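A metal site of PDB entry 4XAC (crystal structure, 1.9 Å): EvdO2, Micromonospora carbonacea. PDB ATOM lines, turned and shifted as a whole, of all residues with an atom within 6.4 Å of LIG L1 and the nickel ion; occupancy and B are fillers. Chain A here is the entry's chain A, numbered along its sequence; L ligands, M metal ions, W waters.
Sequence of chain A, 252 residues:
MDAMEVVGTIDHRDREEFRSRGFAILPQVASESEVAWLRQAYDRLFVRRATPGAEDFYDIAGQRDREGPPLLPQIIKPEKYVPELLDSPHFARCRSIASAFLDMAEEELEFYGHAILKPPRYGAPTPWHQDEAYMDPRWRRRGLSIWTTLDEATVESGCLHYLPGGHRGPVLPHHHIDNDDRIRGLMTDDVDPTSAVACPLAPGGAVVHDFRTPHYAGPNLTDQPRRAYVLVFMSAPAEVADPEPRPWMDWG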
ATOM      1  N   LEU A  72     -33.038   2.352  15.720  1.00  0.00           N
ATOM      2  CA  LEU A  72     -31.914   1.896  14.922  1.00  0.00           C
ATOM      3  C   LEU A  72     -32.372   0.784  13.989  1.00  0.00           C
ATOM      4  O   LEU A  72     -32.907  -0.218  14.465  1.00  0.00           O
ATOM      5  CB  LEU A  72     -30.789   1.415  15.847  1.00  0.00           C
ATOM      6  CG  LEU A  72     -29.471   0.954  15.224  1.00  0.00           C
ATOM      7  CD1 LEU A  72     -28.841   2.089  14.458  1.00  0.00           C
ATOM      8  CD2 LEU A  72     -28.538   0.465  16.323  1.00  0.00           C
ATOM      9  N   HIS A 114     -27.330 -11.003  13.792  1.00  0.00           N
ATOM     10  CA  HIS A 114     -28.049  -9.769  14.049  1.00  0.00           C
ATOM     11  C   HIS A 114     -27.479  -8.720  13.099  1.00  0.00           C
ATOM     12  O   HIS A 114     -26.267  -8.541  13.031  1.00  0.00           O
ATOM     13  CB  HIS A 114     -27.891  -9.360  15.512  1.00  0.00           C
ATOM     14  CG  HIS A 114     -28.612  -8.099  15.882  1.00  0.00           C
ATOM     15  ND1 HIS A 114     -28.138  -7.225  16.830  1.00  0.00           N
ATOM     16  CD2 HIS A 114     -29.763  -7.571  15.421  1.00  0.00           C
ATOM     17  CE1 HIS A 114     -28.970  -6.212  16.953  1.00  0.00           C
ATOM     18  NE2 HIS A 114     -29.971  -6.393  16.097  1.00  0.00           N
ATOM     19  N   ILE A 116     -27.323  -4.749  11.621  1.00  0.00           N
ATOM     20  CA  ILE A 116     -27.544  -3.361  11.978  1.00  0.00           C
ATOM     21  C   ILE A 116     -27.128  -2.479  10.819  1.00  0.00           C
ATOM     22  O   ILE A 116     -26.145  -2.755  10.108  1.00  0.00           O
ATOM     23  CB  ILE A 116     -26.763  -2.965  13.241  1.00  0.00           C
ATOM     24  CG1 ILE A 116     -27.024  -3.949  14.376  1.00  0.00           C
ATOM     25  CG2 ILE A 116     -27.138  -1.560  13.675  1.00  0.00           C
ATOM     26  CD1 ILE A 116     -26.138  -3.739  15.572  1.00  0.00           C
ATOM     27  N   LYS A 118     -26.699   1.715  10.469  1.00  0.00           N
ATOM     28  CA  LYS A 118     -26.814   3.124  10.852  1.00  0.00           C
ATOM     29  C   LYS A 118     -26.870   3.931   9.578  1.00  0.00           C
ATOM     30  O   LYS A 118     -25.848   4.046   8.886  1.00  0.00           O
ATOM     31  CB  LYS A 118     -25.638   3.584  11.723  1.00  0.00           C
ATOM     32  CG  LYS A 118     -25.696   3.100  13.173  1.00  0.00           C
ATOM     33  CD  LYS A 118     -24.751   3.926  14.049  1.00  0.00           C
ATOM     34  CE  LYS A 118     -25.496   4.659  15.177  1.00  0.00           C
ATOM     35  NZ  LYS A 118     -25.738   3.834  16.401  1.00  0.00           N
ATOM     36  N   PRO A 125     -27.149   7.887  19.349  1.00  0.00           N
ATOM     37  CA  PRO A 125     -26.097   6.908  19.647  1.00  0.00           C
ATOM     38  C   PRO A 125     -26.721   5.586  20.014  1.00  0.00           C
ATOM     39  O   PRO A 125     -27.945   5.519  20.177  1.00  0.00           O
ATOM     40  CB  PRO A 125     -25.367   7.522  20.851  1.00  0.00           C
ATOM     41  CG  PRO A 125     -26.496   8.275  21.582  1.00  0.00           C
ATOM     42  CD  PRO A 125     -27.455   8.752  20.510  1.00  0.00           C
ATOM     43  N   THR A 126     -25.920   4.538  20.124  1.00  0.00           N
ATOM     44  CA  THR A 126     -26.338   3.362  20.860  1.00  0.00           C
ATOM     45  C   THR A 126     -25.773   3.579  22.258  1.00  0.00           C
ATOM     46  O   THR A 126     -24.564   3.524  22.452  1.00  0.00           O
ATOM     47  CB  THR A 126     -25.777   2.041  20.264  1.00  0.00           C
ATOM     48  OG1 THR A 126     -26.162   1.937  18.886  1.00  0.00           O
ATOM     49  CG2 THR A 126     -26.316   0.851  21.036  1.00  0.00           C
ATOM     50  N   HIS A 129     -24.323   0.216  27.354  1.00  0.00           N
ATOM     51  CA  HIS A 129     -25.063  -0.946  27.823  1.00  0.00           C
ATOM     52  C   HIS A 129     -24.139  -2.158  27.895  1.00  0.00           C
ATOM     53  O   HIS A 129     -23.045  -2.146  27.316  1.00  0.00           O
ATOM     54  CB  HIS A 129     -26.269  -1.233  26.896  1.00  0.00           C
ATOM     55  CG  HIS A 129     -25.870  -1.782  25.552  1.00  0.00           C
ATOM     56  ND1 HIS A 129     -25.368  -0.971  24.549  1.00  0.00           N
ATOM     57  CD2 HIS A 129     -25.850  -3.043  25.067  1.00  0.00           C
ATOM     58  CE1 HIS A 129     -25.062  -1.718  23.497  1.00  0.00           C
ATOM     59  NE2 HIS A 129     -25.339  -2.983  23.789  1.00  0.00           N
ATOM     60  N   GLN A 130     -24.586  -3.181  28.610  1.00  0.00           N
ATOM     61  CA  GLN A 130     -23.978  -4.493  28.548  1.00  0.00           C
ATOM     62  C   GLN A 130     -24.986  -5.448  27.934  1.00  0.00           C
ATOM     63  O   GLN A 130     -26.174  -5.410  28.252  1.00  0.00           O
ATOM     64  CB  GLN A 130     -23.565  -4.980  29.945  1.00  0.00           C
ATOM     65  CG  GLN A 130     -22.419  -4.203  30.543  1.00  0.00           C
ATOM     66  CD  GLN A 130     -22.440  -4.307  32.047  1.00  0.00           C
ATOM     67  OE1 GLN A 130     -23.384  -3.836  32.690  1.00  0.00           O
ATOM     68  NE2 GLN A 130     -21.444  -4.974  32.602  1.00  0.00           N
ATOM     69  N   ASP A 131     -24.536  -6.304  27.035  1.00  0.00           N
ATOM     70  CA  ASP A 131     -25.463  -7.179  26.331  1.00  0.00           C
ATOM     71  C   ASP A 131     -26.155  -8.130  27.321  1.00  0.00           C
ATOM     72  O   ASP A 131     -27.312  -8.508  27.136  1.00  0.00           O
ATOM     73  CB  ASP A 131     -24.724  -7.947  25.225  1.00  0.00           C
ATOM     74  CG  ASP A 131     -24.228  -7.022  24.119  1.00  0.00           C
ATOM     75  OD1 ASP A 131     -24.785  -5.921  23.964  1.00  0.00           O
ATOM     76  OD2 ASP A 131     -23.271  -7.389  23.402  1.00  0.00           O
ATOM     77  N   TYR A 134     -29.733  -7.621  28.828  1.00  0.00           N
ATOM     78  CA  TYR A 134     -30.934  -8.029  28.103  1.00  0.00           C
ATOM     79  C   TYR A 134     -31.313  -9.469  28.395  1.00  0.00           C
ATOM     80  O   TYR A 134     -32.337  -9.964  27.923  1.00  0.00           O
ATOM     81  CB  TYR A 134     -30.734  -7.869  26.593  1.00  0.00           C
ATOM     82  CG  TYR A 134     -30.755  -6.452  26.089  1.00  0.00           C
ATOM     83  CD1 TYR A 134     -31.956  -5.819  25.757  1.00  0.00           C
ATOM     84  CD2 TYR A 134     -29.565  -5.732  25.897  1.00  0.00           C
ATOM     85  CE1 TYR A 134     -31.982  -4.504  25.277  1.00  0.00           C
ATOM     86  CE2 TYR A 134     -29.591  -4.417  25.417  1.00  0.00           C
ATOM     87  CZ  TYR A 134     -30.799  -3.820  25.107  1.00  0.00           C
ATOM     88  OH  TYR A 134     -30.821  -2.514  24.628  1.00  0.00           O
ATOM     89  N   SER A 145     -19.940 -11.529  21.303  1.00  0.00           N
ATOM     90  CA  SER A 145     -20.480 -11.053  20.042  1.00  0.00           C
ATOM     91  C   SER A 145     -19.332 -10.698  19.122  1.00  0.00           C
ATOM     92  O   SER A 145     -18.367 -10.099  19.567  1.00  0.00           O
ATOM     93  CB  SER A 145     -21.385  -9.838  20.254  1.00  0.00           C
ATOM     94  OG  SER A 145     -22.499 -10.205  21.055  1.00  0.00           O
ATOM     95  N   TRP A 147     -18.723  -8.423  15.955  1.00  0.00           N
ATOM     96  CA  TRP A 147     -19.322  -7.320  15.217  1.00  0.00           C
ATOM     97  C   TRP A 147     -18.467  -7.051  13.987  1.00  0.00           C
ATOM     98  O   TRP A 147     -17.426  -6.422  14.095  1.00  0.00           O
ATOM     99  CB  TRP A 147     -19.386  -6.100  16.155  1.00  0.00           C
ATOM    100  CG  TRP A 147     -20.158  -4.839  15.785  1.00  0.00           C
ATOM    101  CD1 TRP A 147     -21.447  -4.511  16.173  1.00  0.00           C
ATOM    102  CD2 TRP A 147     -19.646  -3.680  15.104  1.00  0.00           C
ATOM    103  NE1 TRP A 147     -21.768  -3.242  15.721  1.00  0.00           N
ATOM    104  CE2 TRP A 147     -20.686  -2.714  15.076  1.00  0.00           C
ATOM    105  CE3 TRP A 147     -18.418  -3.367  14.509  1.00  0.00           C
ATOM    106  CZ2 TRP A 147     -20.532  -1.462  14.466  1.00  0.00           C
ATOM    107  CZ3 TRP A 147     -18.269  -2.106  13.899  1.00  0.00           C
ATOM    108  CH2 TRP A 147     -19.323  -1.191  13.878  1.00  0.00           C
ATOM    109  N   GLY A 158     -19.889   5.888  13.749  1.00  0.00           N
ATOM    110  CA  GLY A 158     -20.545   5.009  14.703  1.00  0.00           C
ATOM    111  C   GLY A 158     -19.837   3.716  15.085  1.00  0.00           C
ATOM    112  O   GLY A 158     -20.499   2.702  15.299  1.00  0.00           O
ATOM    113  N   LEU A 160     -17.716   1.150  17.621  1.00  0.00           N
ATOM    114  CA  LEU A 160     -17.952   0.820  19.021  1.00  0.00           C
ATOM    115  C   LEU A 160     -16.881   1.409  19.932  1.00  0.00           C
ATOM    116  O   LEU A 160     -15.724   1.563  19.536  1.00  0.00           O
ATOM    117  CB  LEU A 160     -18.023  -0.706  19.211  1.00  0.00           C
ATOM    118  CG  LEU A 160     -19.173  -1.383  18.433  1.00  0.00           C
ATOM    119  CD1 LEU A 160     -19.445  -2.813  18.922  1.00  0.00           C
ATOM    120  CD2 LEU A 160     -20.451  -0.551  18.524  1.00  0.00           C
ATOM    121  N   HIS A 209     -16.679  -8.765  21.630  1.00  0.00           N
ATOM    122  CA  HIS A 209     -16.792  -8.428  23.044  1.00  0.00           C
ATOM    123  C   HIS A 209     -17.625  -9.416  23.851  1.00  0.00           C
ATOM    124  O   HIS A 209     -18.605  -9.980  23.362  1.00  0.00           O
ATOM    125  CB  HIS A 209     -17.355  -6.996  23.248  1.00  0.00           C
ATOM    126  CG  HIS A 209     -18.698  -6.752  22.637  1.00  0.00           C
ATOM    127  ND1 HIS A 209     -18.861  -6.177  21.392  1.00  0.00           N
ATOM    128  CD2 HIS A 209     -19.954  -6.940  23.127  1.00  0.00           C
ATOM    129  CE1 HIS A 209     -20.144  -6.063  21.121  1.00  0.00           C
ATOM    130  NE2 HIS A 209     -20.833  -6.518  22.154  1.00  0.00           N
ATOM    131  N   HIS A 215     -20.416  -1.298  26.334  1.00  0.00           N
ATOM    132  CA  HIS A 215     -20.098  -0.651  25.063  1.00  0.00           C
ATOM    133  C   HIS A 215     -21.150   0.353  24.630  1.00  0.00           C
ATOM    134  O   HIS A 215     -22.293   0.368  25.113  1.00  0.00           O
ATOM    135  CB  HIS A 215     -19.865  -1.706  23.967  1.00  0.00           C
ATOM    136  CG  HIS A 215     -20.991  -2.683  23.801  1.00  0.00           C
ATOM    137  ND1 HIS A 215     -21.199  -3.735  24.665  1.00  0.00           N
ATOM    138  CD2 HIS A 215     -21.945  -2.791  22.846  1.00  0.00           C
ATOM    139  CE1 HIS A 215     -22.245  -4.428  24.261  1.00  0.00           C
ATOM    140  NE2 HIS A 215     -22.718  -3.877  23.170  1.00  0.00           N
ATOM    141  N   TYR A 216     -20.728   1.207  23.699  1.00  0.00           N
ATOM    142  CA  TYR A 216     -21.467   2.378  23.248  1.00  0.00           C
ATOM    143  C   TYR A 216     -21.140   2.582  21.779  1.00  0.00           C
ATOM    144  O   TYR A 216     -20.012   2.261  21.353  1.00  0.00           O
ATOM    145  CB  TYR A 216     -21.058   3.594  24.077  1.00  0.00           C
ATOM    146  CG  TYR A 216     -21.364   4.941  23.467  1.00  0.00           C
ATOM    147  CD1 TYR A 216     -20.454   5.560  22.605  1.00  0.00           C
ATOM    148  CD2 TYR A 216     -22.528   5.607  23.789  1.00  0.00           C
ATOM    149  CE1 TYR A 216     -20.721   6.807  22.064  1.00  0.00           C
ATOM    150  CE2 TYR A 216     -22.805   6.860  23.240  1.00  0.00           C
ATOM    151  CZ  TYR A 216     -21.889   7.450  22.386  1.00  0.00           C
ATOM    152  OH  TYR A 216     -22.146   8.678  21.832  1.00  0.00           O
ATOM    153  N   ALA A 217     -22.088   3.092  20.997  1.00  0.00           N
ATOM    154  CA  ALA A 217     -21.778   3.495  19.627  1.00  0.00           C
ATOM    155  C   ALA A 217     -22.257   4.921  19.382  1.00  0.00           C
ATOM    156  O   ALA A 217     -23.393   5.265  19.693  1.00  0.00           O
ATOM    157  CB  ALA A 217     -22.402   2.530  18.610  1.00  0.00           C
ATOM    158  N   GLY A 218     -21.387   5.751  18.823  1.00  0.00           N
ATOM    159  CA  GLY A 218     -21.755   7.118  18.528  1.00  0.00           C
ATOM    160  C   GLY A 218     -22.719   7.218  17.361  1.00  0.00           C
ATOM    161  O   GLY A 218     -23.006   6.219  16.703  1.00  0.00           O
ATOM    162  N   ALA A 228     -23.276  -3.218   9.951  1.00  0.00           N
ATOM    163  CA  ALA A 228     -22.553  -4.211  10.742  1.00  0.00           C
ATOM    164  C   ALA A 228     -23.349  -5.494  10.766  1.00  0.00           C
ATOM    165  O   ALA A 228     -24.592  -5.479  10.741  1.00  0.00           O
ATOM    166  CB  ALA A 228     -22.306  -3.725  12.164  1.00  0.00           C
ATOM    167  N   VAL A 230     -23.552  -8.883  13.025  1.00  0.00           N
ATOM    168  CA  VAL A 230     -23.105  -9.381  14.317  1.00  0.00           C
ATOM    169  C   VAL A 230     -23.422 -10.854  14.451  1.00  0.00           C
ATOM    170  O   VAL A 230     -24.526 -11.280  14.135  1.00  0.00           O
ATOM    171  CB  VAL A 230     -23.759  -8.612  15.478  1.00  0.00           C
ATOM    172  CG1 VAL A 230     -23.100  -9.001  16.807  1.00  0.00           C
ATOM    173  CG2 VAL A 230     -23.624  -7.101  15.255  1.00  0.00           C
HETATM  174  C1  LIG L   1     -23.676  -5.097  20.010  1.00  0.00           C
HETATM  175  O1  LIG L   1     -23.196  -5.643  18.982  1.00  0.00           O
HETATM  176  O2  LIG L   1     -23.828  -5.728  21.083  1.00  0.00           O
HETATM  177  C2  LIG L   1     -24.096  -3.664  19.959  1.00  0.00           C
HETATM  178  O3  LIG L   1     -24.654  -3.149  20.926  1.00  0.00           O
HETATM  179  C3  LIG L   1     -23.871  -2.883  18.714  1.00  0.00           C
HETATM  180  C4  LIG L   1     -24.297  -1.452  18.684  1.00  0.00           C
HETATM  181  C5  LIG L   1     -24.230  -0.730  17.377  1.00  0.00           C
HETATM  182  O4  LIG L   1     -23.820  -1.323  16.347  1.00  0.00           O
HETATM  183  O5  LIG L   1     -24.569   0.484  17.294  1.00  0.00           O
HETATM  184  N1  LG2 L   2     -28.483  -5.850  21.977  1.00  0.00           N
HETATM  185  C1  LG2 L   2     -27.258  -5.874  22.568  1.00  0.00           C
HETATM  186  N2  LG2 L   2     -26.428  -5.048  21.894  1.00  0.00           N
HETATM  187  C2  LG2 L   2     -27.123  -4.502  20.877  1.00  0.00           C
HETATM  188  C3  LG2 L   2     -28.418  -5.003  20.928  1.00  0.00           C
HETATM  189 NI    NI M   1     -24.612  -4.471  22.520  1.00  0.00          NI
HETATM  190  O   HOH W   1     -24.632  -8.467  20.598  1.00  0.00           O
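Of the 21 residues printed, 3 come within 4 Å of the nickel ion.
Along chain A the residues within 4 Å of the nickel ion span positions 129 to 215.
The side-chain hydroxyl (OG1) of Thr 126 lies within hydrogen-bond range of an oxygen (O5) of LIG L1.
The indole nitrogen of Trp 147 is in hydrogen-bond range of an oxygen (O4) of LIG L1, 2.9 Å away.
NE2 of His 209 lies close to O2 of LIG L1, 3.3 Å away.
O5 of LIG L1 lies within salt-bridge range of NZ of Lys 118, 3.7 Å away.
N2 of LG2 L2 is bound to the nickel ion.
OD1 of Asp 131 is bound to the nickel ion (2.1 Å).
The nickel ion is bound by O2 of LIG L1, 2.1 Å away.
O3 of LIG L1 binds the nickel ion (2.1 Å).
NE2 of His 129 is bound to the nickel ion (2.1 Å).
NE2 of His 215 is bound to the nickel ion (2.1 Å).
Residues that only touch LIG L1: Ala 217 (3.3 Å), Ile 116 (3.4 Å) and Leu 160 (3.95 Å).
Hydrophobic or aromatic side chains within 4 Å of LIG L1: Ile 116, His 129, Trp 147, Leu 160, His 209, His 215 and Ala 217.
Of the 21 residues printed, 10 come within 4 Å of LIG L1.
Water W1 lies within hydrogen-bond range of OG of Ser 145 (2.8 Å) and OD2 of Asp 131 (3.3 Å).
OD2 of Asp 131 sits at hydrogen-bond distance from NE2 of His 209 (2.9 Å).
A ring nitrogen (NE2) of His 215 sits close to a ring nitrogen (NE2) of His 209 (3.4 Å).
N of Thr 126 sits at hydrogen-bond distance from O of Ala 217 (2.7 Å).
OG1 of Thr 126 is in hydrogen-bond range of NZ of Lys 118, at 3.2 Å.
The backbone carbonyl oxygen (O) of His 209 sits at hydrogen-bond distance from the backbone NH (N) of Ser 145, at 2.9 Å.
O of Ile 116 is in hydrogen-bond range of N of Ala 228.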
